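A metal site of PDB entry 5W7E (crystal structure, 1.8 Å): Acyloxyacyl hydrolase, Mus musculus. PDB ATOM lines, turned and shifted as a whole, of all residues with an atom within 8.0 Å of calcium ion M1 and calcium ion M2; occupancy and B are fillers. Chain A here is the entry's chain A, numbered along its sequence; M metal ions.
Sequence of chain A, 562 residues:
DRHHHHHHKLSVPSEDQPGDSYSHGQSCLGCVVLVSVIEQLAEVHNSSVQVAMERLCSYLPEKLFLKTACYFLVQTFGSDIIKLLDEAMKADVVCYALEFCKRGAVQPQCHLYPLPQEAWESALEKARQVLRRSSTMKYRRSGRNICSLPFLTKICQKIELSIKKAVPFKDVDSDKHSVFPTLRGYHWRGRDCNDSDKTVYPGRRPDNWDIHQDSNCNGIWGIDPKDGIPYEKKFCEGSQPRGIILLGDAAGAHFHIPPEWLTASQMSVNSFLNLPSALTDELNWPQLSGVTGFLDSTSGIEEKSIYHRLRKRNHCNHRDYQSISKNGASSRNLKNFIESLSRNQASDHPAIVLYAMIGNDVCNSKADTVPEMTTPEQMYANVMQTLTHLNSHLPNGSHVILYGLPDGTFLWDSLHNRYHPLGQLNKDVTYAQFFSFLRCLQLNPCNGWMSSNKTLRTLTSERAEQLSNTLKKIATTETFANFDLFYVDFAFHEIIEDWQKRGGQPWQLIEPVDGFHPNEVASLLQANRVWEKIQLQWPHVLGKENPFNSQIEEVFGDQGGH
The side-chain amide nitrogen (ND2) of Asn 194 is in hydrogen-bond range of the side-chain amide oxygen (OE1) of Gln 213 (2.9 Å). OD1 of Asn 194 lies within hydrogen-bond range of N of Ser 196 (3.0 Å). The backbone NH (N) of Lys 176 lies within hydrogen-bond range of the side-chain carboxylate (OD1) of Asp 171 (2.8 Å). The side-chain hydroxyl (OG1) of Thr 199 is in hydrogen-bond range of the side-chain carboxylate (OD1) of Asp 197, 2.6 Å away. N of Lys 198 lies close to OD2 of Asp 173 (3.4 Å). N of Ser 174 lies close to OD2 of Asp 171 (3.2 Å). The side-chain sulfur (SG) of Cys 217 is disulfide-bonded to the side-chain sulfur (SG) of Cys 193 (2.1 Å). The side-chain carboxylate (OD2) of Asp 195 is in hydrogen-bond range of the backbone NH (N) of Val 172 (3.0 Å).
Of the 27 residues printed, 6 come within 4 Å of calcium ion M1.
Of the 27 residues printed, 6 come within 4 Å of calcium ion M2. The nearest printed residue that does not touch calcium ion M2 is Asp 195 (4.05 Å).
Calcium ion M1 is bound by the side-chain carboxylate (OD2) of Asp 171 (2.2 Å), the side-chain carboxylate (OD1) of Asp 195 (2.3 Å), the side-chain carboxylate (OD2) of Asp 192 (2.3 Å), the side-chain carboxylate (OD1) of Asp 175 (2.3 Å), the backbone carbonyl oxygen (O) of His 177 (2.3 Å) and the side-chain carboxylate (OD1) of Asp 173 (2.3 Å).
Calcium ion M2 is bound by the side-chain carboxylate (OD2) of Asp 175 (2.2 Å), the backbone carbonyl oxygen (O) of Val 200 (2.3 Å), the backbone carbonyl oxygen (O) of Asn 194 (2.3 Å), the side-chain carboxylate (OD2) of Asp 173 (2.3 Å), the backbone carbonyl oxygen (O) of Asp 197 (2.5 Å), the side-chain carboxylate (OD2) of Asp 192 (2.5 Å) and the side-chain carboxylate (OD1) of Asp 192 (2.6 Å).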
ATOM      1  N   PRO A 168       1.708 -22.671 -37.603  1.00  0.00           N
ATOM      2  CA  PRO A 168       1.595 -21.389 -36.923  1.00  0.00           C
ATOM      3  C   PRO A 168       2.925 -20.896 -36.374  1.00  0.00           C
ATOM      4  O   PRO A 168       3.691 -21.653 -35.768  1.00  0.00           O
ATOM      5  CB  PRO A 168       0.599 -21.675 -35.792  1.00  0.00           C
ATOM      6  CG  PRO A 168       0.614 -23.151 -35.646  1.00  0.00           C
ATOM      7  CD  PRO A 168       0.795 -23.664 -37.020  1.00  0.00           C
ATOM      8  N   LYS A 170       3.164 -18.627 -33.958  1.00  0.00           N
ATOM      9  CA  LYS A 170       2.977 -18.611 -32.503  1.00  0.00           C
ATOM     10  C   LYS A 170       2.364 -19.952 -32.094  1.00  0.00           C
ATOM     11  O   LYS A 170       1.189 -20.213 -32.356  1.00  0.00           O
ATOM     12  CB  LYS A 170       2.083 -17.449 -32.085  1.00  0.00           C
ATOM     13  CG  LYS A 170       2.478 -16.101 -32.653  1.00  0.00           C
ATOM     14  CD  LYS A 170       3.536 -15.377 -31.844  1.00  0.00           C
ATOM     15  CE  LYS A 170       3.140 -13.909 -31.581  1.00  0.00           C
ATOM     16  NZ  LYS A 170       2.830 -13.098 -32.815  1.00  0.00           N
ATOM     17  N   ASP A 171       3.169 -20.793 -31.434  1.00  0.00           N
ATOM     18  CA  ASP A 171       2.789 -22.151 -31.078  1.00  0.00           C
ATOM     19  C   ASP A 171       3.785 -22.694 -30.063  1.00  0.00           C
ATOM     20  O   ASP A 171       4.692 -23.458 -30.406  1.00  0.00           O
ATOM     21  CB  ASP A 171       2.709 -22.998 -32.350  1.00  0.00           C
ATOM     22  CG  ASP A 171       2.203 -24.406 -32.101  1.00  0.00           C
ATOM     23  OD1 ASP A 171       2.479 -25.244 -32.990  1.00  0.00           O
ATOM     24  OD2 ASP A 171       1.555 -24.679 -31.040  1.00  0.00           O
ATOM     25  N   VAL A 172       3.604 -22.303 -28.789  1.00  0.00           N
ATOM     26  CA  VAL A 172       4.580 -22.604 -27.740  1.00  0.00           C
ATOM     27  C   VAL A 172       4.754 -24.110 -27.594  1.00  0.00           C
ATOM     28  O   VAL A 172       5.886 -24.593 -27.454  1.00  0.00           O
ATOM     29  CB  VAL A 172       4.161 -21.967 -26.419  1.00  0.00           C
ATOM     30  CG1 VAL A 172       5.024 -22.480 -25.253  1.00  0.00           C
ATOM     31  CG2 VAL A 172       4.268 -20.483 -26.518  1.00  0.00           C
ATOM     32  N   ASP A 173       3.651 -24.863 -27.578  1.00  0.00           N
ATOM     33  CA  ASP A 173       3.744 -26.301 -27.348  1.00  0.00           C
ATOM     34  C   ASP A 173       3.852 -27.105 -28.637  1.00  0.00           C
ATOM     35  O   ASP A 173       3.821 -28.343 -28.576  1.00  0.00           O
ATOM     36  CB  ASP A 173       2.548 -26.801 -26.520  1.00  0.00           C
ATOM     37  CG  ASP A 173       1.241 -26.630 -27.248  1.00  0.00           C
ATOM     38  OD1 ASP A 173       1.277 -26.288 -28.439  1.00  0.00           O
ATOM     39  OD2 ASP A 173       0.190 -26.834 -26.610  1.00  0.00           O
ATOM     40  N   SER A 174       3.944 -26.435 -29.789  1.00  0.00           N
ATOM     41  CA  SER A 174       4.280 -27.056 -31.077  1.00  0.00           C
ATOM     42  C   SER A 174       3.236 -28.051 -31.568  1.00  0.00           C
ATOM     43  O   SER A 174       3.563 -28.930 -32.378  1.00  0.00           O
ATOM     44  CB  SER A 174       5.652 -27.731 -31.024  1.00  0.00           C
ATOM     45  OG  SER A 174       6.703 -26.779 -30.880  1.00  0.00           O
ATOM     46  N   ASP A 175       1.978 -27.965 -31.126  1.00  0.00           N
ATOM     47  CA  ASP A 175       0.956 -28.902 -31.609  1.00  0.00           C
ATOM     48  C   ASP A 175       0.242 -28.402 -32.869  1.00  0.00           C
ATOM     49  O   ASP A 175      -0.755 -29.007 -33.277  1.00  0.00           O
ATOM     50  CB  ASP A 175      -0.041 -29.252 -30.484  1.00  0.00           C
ATOM     51  CG  ASP A 175      -0.791 -28.060 -29.923  1.00  0.00           C
ATOM     52  OD1 ASP A 175      -0.793 -26.980 -30.566  1.00  0.00           O
ATOM     53  OD2 ASP A 175      -1.383 -28.213 -28.818  1.00  0.00           O
ATOM     54  N   LYS A 176       0.748 -27.334 -33.494  1.00  0.00           N
ATOM     55  CA  LYS A 176       0.261 -26.733 -34.747  1.00  0.00           C
ATOM     56  C   LYS A 176      -1.062 -25.990 -34.588  1.00  0.00           C
ATOM     57  O   LYS A 176      -1.667 -25.567 -35.594  1.00  0.00           O
ATOM     58  CB  LYS A 176       0.145 -27.784 -35.859  1.00  0.00           C
ATOM     59  CG  LYS A 176       1.516 -28.326 -36.293  1.00  0.00           C
ATOM     60  CD  LYS A 176       1.430 -29.362 -37.397  1.00  0.00           C
ATOM     61  CE  LYS A 176       2.772 -30.014 -37.669  1.00  0.00           C
ATOM     62  NZ  LYS A 176       3.309 -30.720 -36.461  1.00  0.00           N
ATOM     63  N   HIS A 177      -1.530 -25.775 -33.355  1.00  0.00           N
ATOM     64  CA  HIS A 177      -2.691 -24.957 -33.073  1.00  0.00           C
ATOM     65  C   HIS A 177      -2.248 -23.751 -32.260  1.00  0.00           C
ATOM     66  O   HIS A 177      -1.418 -23.874 -31.359  1.00  0.00           O
ATOM     67  CB  HIS A 177      -3.777 -25.773 -32.333  1.00  0.00           C
ATOM     68  CG  HIS A 177      -4.377 -26.840 -33.177  1.00  0.00           C
ATOM     69  ND1 HIS A 177      -5.533 -26.655 -33.903  1.00  0.00           N
ATOM     70  CD2 HIS A 177      -3.960 -28.104 -33.442  1.00  0.00           C
ATOM     71  CE1 HIS A 177      -5.815 -27.760 -34.562  1.00  0.00           C
ATOM     72  NE2 HIS A 177      -4.880 -28.653 -34.300  1.00  0.00           N
ATOM     73  N   SER A 178      -2.807 -22.597 -32.580  1.00  0.00           N
ATOM     74  CA  SER A 178      -2.315 -21.331 -32.063  1.00  0.00           C
ATOM     75  C   SER A 178      -3.370 -20.609 -31.232  1.00  0.00           C
ATOM     76  O   SER A 178      -4.569 -20.875 -31.321  1.00  0.00           O
ATOM     77  CB  SER A 178      -1.880 -20.447 -33.232  1.00  0.00           C
ATOM     78  OG  SER A 178      -1.238 -19.248 -32.817  1.00  0.00           O
ATOM     79  N   VAL A 179      -2.888 -19.663 -30.416  1.00  0.00           N
ATOM     80  CA  VAL A 179      -3.757 -18.693 -29.746  1.00  0.00           C
ATOM     81  C   VAL A 179      -3.811 -17.368 -30.494  1.00  0.00           C
ATOM     82  O   VAL A 179      -4.547 -16.459 -30.092  1.00  0.00           O
ATOM     83  CB  VAL A 179      -3.311 -18.461 -28.287  1.00  0.00           C
ATOM     84  CG1 VAL A 179      -3.140 -19.768 -27.568  1.00  0.00           C
ATOM     85  CG2 VAL A 179      -2.010 -17.662 -28.237  1.00  0.00           C
ATOM     86  N   GLY A 190      -8.512 -24.761 -35.571  1.00  0.00           N
ATOM     87  CA  GLY A 190      -9.071 -24.531 -34.269  1.00  0.00           C
ATOM     88  C   GLY A 190      -8.085 -23.934 -33.280  1.00  0.00           C
ATOM     89  O   GLY A 190      -6.930 -24.372 -33.207  1.00  0.00           O
ATOM     90  N   ARG A 191      -8.549 -22.939 -32.541  1.00  0.00           N
ATOM     91  CA  ARG A 191      -7.733 -22.247 -31.552  1.00  0.00           C
ATOM     92  C   ARG A 191      -7.329 -23.194 -30.424  1.00  0.00           C
ATOM     93  O   ARG A 191      -8.156 -23.948 -29.905  1.00  0.00           O
ATOM     94  CB  ARG A 191      -8.505 -21.049 -30.994  1.00  0.00           C
ATOM     95  CG  ARG A 191      -7.621 -20.098 -30.161  1.00  0.00           C
ATOM     96  CD  ARG A 191      -8.417 -19.242 -29.209  1.00  0.00           C
ATOM     97  NE  ARG A 191      -9.345 -18.342 -29.887  1.00  0.00           N
ATOM     98  CZ  ARG A 191      -9.283 -17.007 -29.892  1.00  0.00           C
ATOM     99  NH1 ARG A 191      -8.323 -16.360 -29.243  1.00  0.00           N
ATOM    100  NH2 ARG A 191     -10.192 -16.304 -30.532  1.00  0.00           N
ATOM    101  N   ASP A 192      -6.052 -23.161 -30.057  1.00  0.00           N
ATOM    102  CA  ASP A 192      -5.511 -23.969 -28.953  1.00  0.00           C
ATOM    103  C   ASP A 192      -6.035 -23.460 -27.621  1.00  0.00           C
ATOM    104  O   ASP A 192      -5.750 -22.322 -27.237  1.00  0.00           O
ATOM    105  CB  ASP A 192      -3.985 -23.912 -28.974  1.00  0.00           C
ATOM    106  CG  ASP A 192      -3.339 -25.027 -28.205  1.00  0.00           C
ATOM    107  OD1 ASP A 192      -4.032 -25.666 -27.381  1.00  0.00           O
ATOM    108  OD2 ASP A 192      -2.116 -25.243 -28.427  1.00  0.00           O
ATOM    109  N   CYS A 193      -6.766 -24.306 -26.896  1.00  0.00           N
ATOM    110  CA  CYS A 193      -7.263 -23.942 -25.576  1.00  0.00           C
ATOM    111  C   CYS A 193      -6.159 -23.970 -24.513  1.00  0.00           C
ATOM    112  O   CYS A 193      -6.285 -23.291 -23.480  1.00  0.00           O
ATOM    113  CB  CYS A 193      -8.451 -24.844 -25.166  1.00  0.00           C
ATOM    114  SG  CYS A 193      -8.272 -26.679 -25.334  1.00  0.00           S
ATOM    115  N   ASN A 194      -5.074 -24.697 -24.749  1.00  0.00           N
ATOM    116  CA  ASN A 194      -3.919 -24.692 -23.841  1.00  0.00           C
ATOM    117  C   ASN A 194      -2.653 -24.798 -24.675  1.00  0.00           C
ATOM    118  O   ASN A 194      -2.277 -25.892 -25.098  1.00  0.00           O
ATOM    119  CB  ASN A 194      -4.023 -25.824 -22.824  1.00  0.00           C
ATOM    120  CG  ASN A 194      -3.048 -25.634 -21.669  1.00  0.00           C
ATOM    121  OD1 ASN A 194      -2.039 -24.957 -21.835  1.00  0.00           O
ATOM    122  ND2 ASN A 194      -3.368 -26.215 -20.516  1.00  0.00           N
ATOM    123  N   ASP A 195      -1.988 -23.670 -24.916  1.00  0.00           N
ATOM    124  CA  ASP A 195      -0.771 -23.630 -25.708  1.00  0.00           C
ATOM    125  C   ASP A 195       0.461 -24.029 -24.899  1.00  0.00           C
ATOM    126  O   ASP A 195       1.586 -23.926 -25.408  1.00  0.00           O
ATOM    127  CB  ASP A 195      -0.589 -22.245 -26.309  1.00  0.00           C
ATOM    128  CG  ASP A 195       0.344 -22.238 -27.512  1.00  0.00           C
ATOM    129  OD1 ASP A 195       0.358 -23.220 -28.293  1.00  0.00           O
ATOM    130  OD2 ASP A 195       1.059 -21.228 -27.700  1.00  0.00           O
ATOM    131  N   SER A 196       0.264 -24.456 -23.646  1.00  0.00           N
ATOM    132  CA  SER A 196       1.301 -25.018 -22.798  1.00  0.00           C
ATOM    133  C   SER A 196       1.092 -26.507 -22.580  1.00  0.00           C
ATOM    134  O   SER A 196       1.469 -27.046 -21.547  1.00  0.00           O
ATOM    135  CB  SER A 196       1.349 -24.304 -21.438  1.00  0.00           C
ATOM    136  OG  SER A 196       1.430 -22.897 -21.597  1.00  0.00           O
ATOM    137  N   ASP A 197       0.455 -27.177 -23.536  1.00  0.00           N
ATOM    138  CA  ASP A 197       0.219 -28.621 -23.397  1.00  0.00           C
ATOM    139  C   ASP A 197      -0.015 -29.178 -24.789  1.00  0.00           C
ATOM    140  O   ASP A 197      -1.079 -28.949 -25.372  1.00  0.00           O
ATOM    141  CB  ASP A 197      -0.957 -28.899 -22.474  1.00  0.00           C
ATOM    142  CG  ASP A 197      -1.080 -30.373 -22.108  1.00  0.00           C
ATOM    143  OD1 ASP A 197      -0.617 -31.222 -22.911  1.00  0.00           O
ATOM    144  OD2 ASP A 197      -1.628 -30.677 -21.021  1.00  0.00           O
ATOM    145  N   LYS A 198       0.973 -29.909 -25.299  1.00  0.00           N
ATOM    146  CA  LYS A 198       0.909 -30.499 -26.629  1.00  0.00           C
ATOM    147  C   LYS A 198      -0.099 -31.643 -26.733  1.00  0.00           C
ATOM    148  O   LYS A 198      -0.334 -32.138 -27.837  1.00  0.00           O
ATOM    149  CB  LYS A 198       2.297 -30.979 -27.042  1.00  0.00           C
ATOM    150  CG  LYS A 198       2.879 -32.093 -26.181  1.00  0.00           C
ATOM    151  CD  LYS A 198       4.182 -32.634 -26.760  1.00  0.00           C
ATOM    152  CE  LYS A 198       4.545 -34.019 -26.202  1.00  0.00           C
ATOM    153  NZ  LYS A 198       5.099 -33.963 -24.808  1.00  0.00           N
ATOM    154  N   THR A 199      -0.708 -32.067 -25.645  1.00  0.00           N
ATOM    155  CA  THR A 199      -1.753 -33.082 -25.721  1.00  0.00           C
ATOM    156  C   THR A 199      -3.142 -32.492 -25.631  1.00  0.00           C
ATOM    157  O   THR A 199      -4.125 -33.242 -25.601  1.00  0.00           O
ATOM    158  CB  THR A 199      -1.561 -34.137 -24.616  1.00  0.00           C
ATOM    159  OG1 THR A 199      -1.700 -33.525 -23.333  1.00  0.00           O
ATOM    160  CG2 THR A 199      -0.190 -34.781 -24.738  1.00  0.00           C
ATOM    161  N   VAL A 200      -3.248 -31.171 -25.597  1.00  0.00           N
ATOM    162  CA  VAL A 200      -4.514 -30.449 -25.590  1.00  0.00           C
ATOM    163  C   VAL A 200      -4.593 -29.668 -26.896  1.00  0.00           C
ATOM    164  O   VAL A 200      -3.775 -28.766 -27.130  1.00  0.00           O
ATOM    165  CB  VAL A 200      -4.619 -29.494 -24.390  1.00  0.00           C
ATOM    166  CG1 VAL A 200      -5.868 -28.650 -24.496  1.00  0.00           C
ATOM    167  CG2 VAL A 200      -4.618 -30.284 -23.073  1.00  0.00           C
ATOM    168  N   TYR A 201      -5.554 -30.015 -27.740  1.00  0.00           N
ATOM    169  CA  TYR A 201      -5.756 -29.357 -29.029  1.00  0.00           C
ATOM    170  C   TYR A 201      -7.030 -29.921 -29.662  1.00  0.00           C
ATOM    171  O   TYR A 201      -7.426 -31.055 -29.360  1.00  0.00           O
ATOM    172  CB  TYR A 201      -4.558 -29.580 -29.968  1.00  0.00           C
ATOM    173  CG  TYR A 201      -4.231 -31.042 -30.181  1.00  0.00           C
ATOM    174  CD1 TYR A 201      -4.969 -31.830 -31.064  1.00  0.00           C
ATOM    175  CD2 TYR A 201      -3.200 -31.650 -29.480  1.00  0.00           C
ATOM    176  CE1 TYR A 201      -4.681 -33.172 -31.248  1.00  0.00           C
ATOM    177  CE2 TYR A 201      -2.906 -32.983 -29.657  1.00  0.00           C
ATOM    178  CZ  TYR A 201      -3.654 -33.736 -30.538  1.00  0.00           C
ATOM    179  OH  TYR A 201      -3.351 -35.071 -30.718  1.00  0.00           O
ATOM    180  N   PRO A 202      -7.655 -29.174 -30.586  1.00  0.00           N
ATOM    181  CA  PRO A 202      -8.888 -29.667 -31.231  1.00  0.00           C
ATOM    182  C   PRO A 202      -8.688 -30.965 -31.990  1.00  0.00           C
ATOM    183  O   PRO A 202      -7.705 -31.146 -32.711  1.00  0.00           O
ATOM    184  CB  PRO A 202      -9.263 -28.515 -32.169  1.00  0.00           C
ATOM    185  CG  PRO A 202      -8.600 -27.326 -31.610  1.00  0.00           C
ATOM    186  CD  PRO A 202      -7.331 -27.799 -30.986  1.00  0.00           C
ATOM    187  N   GLN A 213      -9.935 -31.419 -17.463  1.00  0.00           N
ATOM    188  CA  GLN A 213      -9.543 -30.416 -18.438  1.00  0.00           C
ATOM    189  C   GLN A 213     -10.250 -30.693 -19.752  1.00  0.00           C
ATOM    190  O   GLN A 213     -10.546 -31.842 -20.098  1.00  0.00           O
ATOM    191  CB  GLN A 213      -8.017 -30.404 -18.651  1.00  0.00           C
ATOM    192  CG  GLN A 213      -7.587 -29.253 -19.567  1.00  0.00           C
ATOM    193  CD  GLN A 213      -6.075 -29.061 -19.678  1.00  0.00           C
ATOM    194  OE1 GLN A 213      -5.622 -28.017 -20.161  1.00  0.00           O
ATOM    195  NE2 GLN A 213      -5.299 -30.061 -19.244  1.00  0.00           N
ATOM    196  N   SER A 215      -9.529 -31.274 -22.898  1.00  0.00           N
ATOM    197  CA  SER A 215      -8.334 -31.661 -23.649  1.00  0.00           C
ATOM    198  C   SER A 215      -8.496 -31.536 -25.165  1.00  0.00           C
ATOM    199  O   SER A 215      -7.483 -31.503 -25.872  1.00  0.00           O
ATOM    200  CB  SER A 215      -7.914 -33.086 -23.285  1.00  0.00           C
ATOM    201  OG  SER A 215      -8.849 -34.038 -23.792  1.00  0.00           O
ATOM    202  N   CYS A 217     -10.571 -29.067 -26.665  1.00  0.00           N
ATOM    203  CA  CYS A 217     -10.922 -27.685 -26.990  1.00  0.00           C
ATOM    204  C   CYS A 217     -12.320 -27.513 -27.549  1.00  0.00           C
ATOM    205  O   CYS A 217     -12.623 -26.475 -28.151  1.00  0.00           O
ATOM    206  CB  CYS A 217      -9.912 -27.082 -27.976  1.00  0.00           C
ATOM    207  SG  CYS A 217      -8.226 -27.174 -27.380  1.00  0.00           S
HETATM  208 CA    CA M   1      -0.206 -24.947 -29.668  1.00  0.00          CA
HETATM  209 CA    CA M   2      -2.079 -27.264 -26.915  1.00  0.00          CA
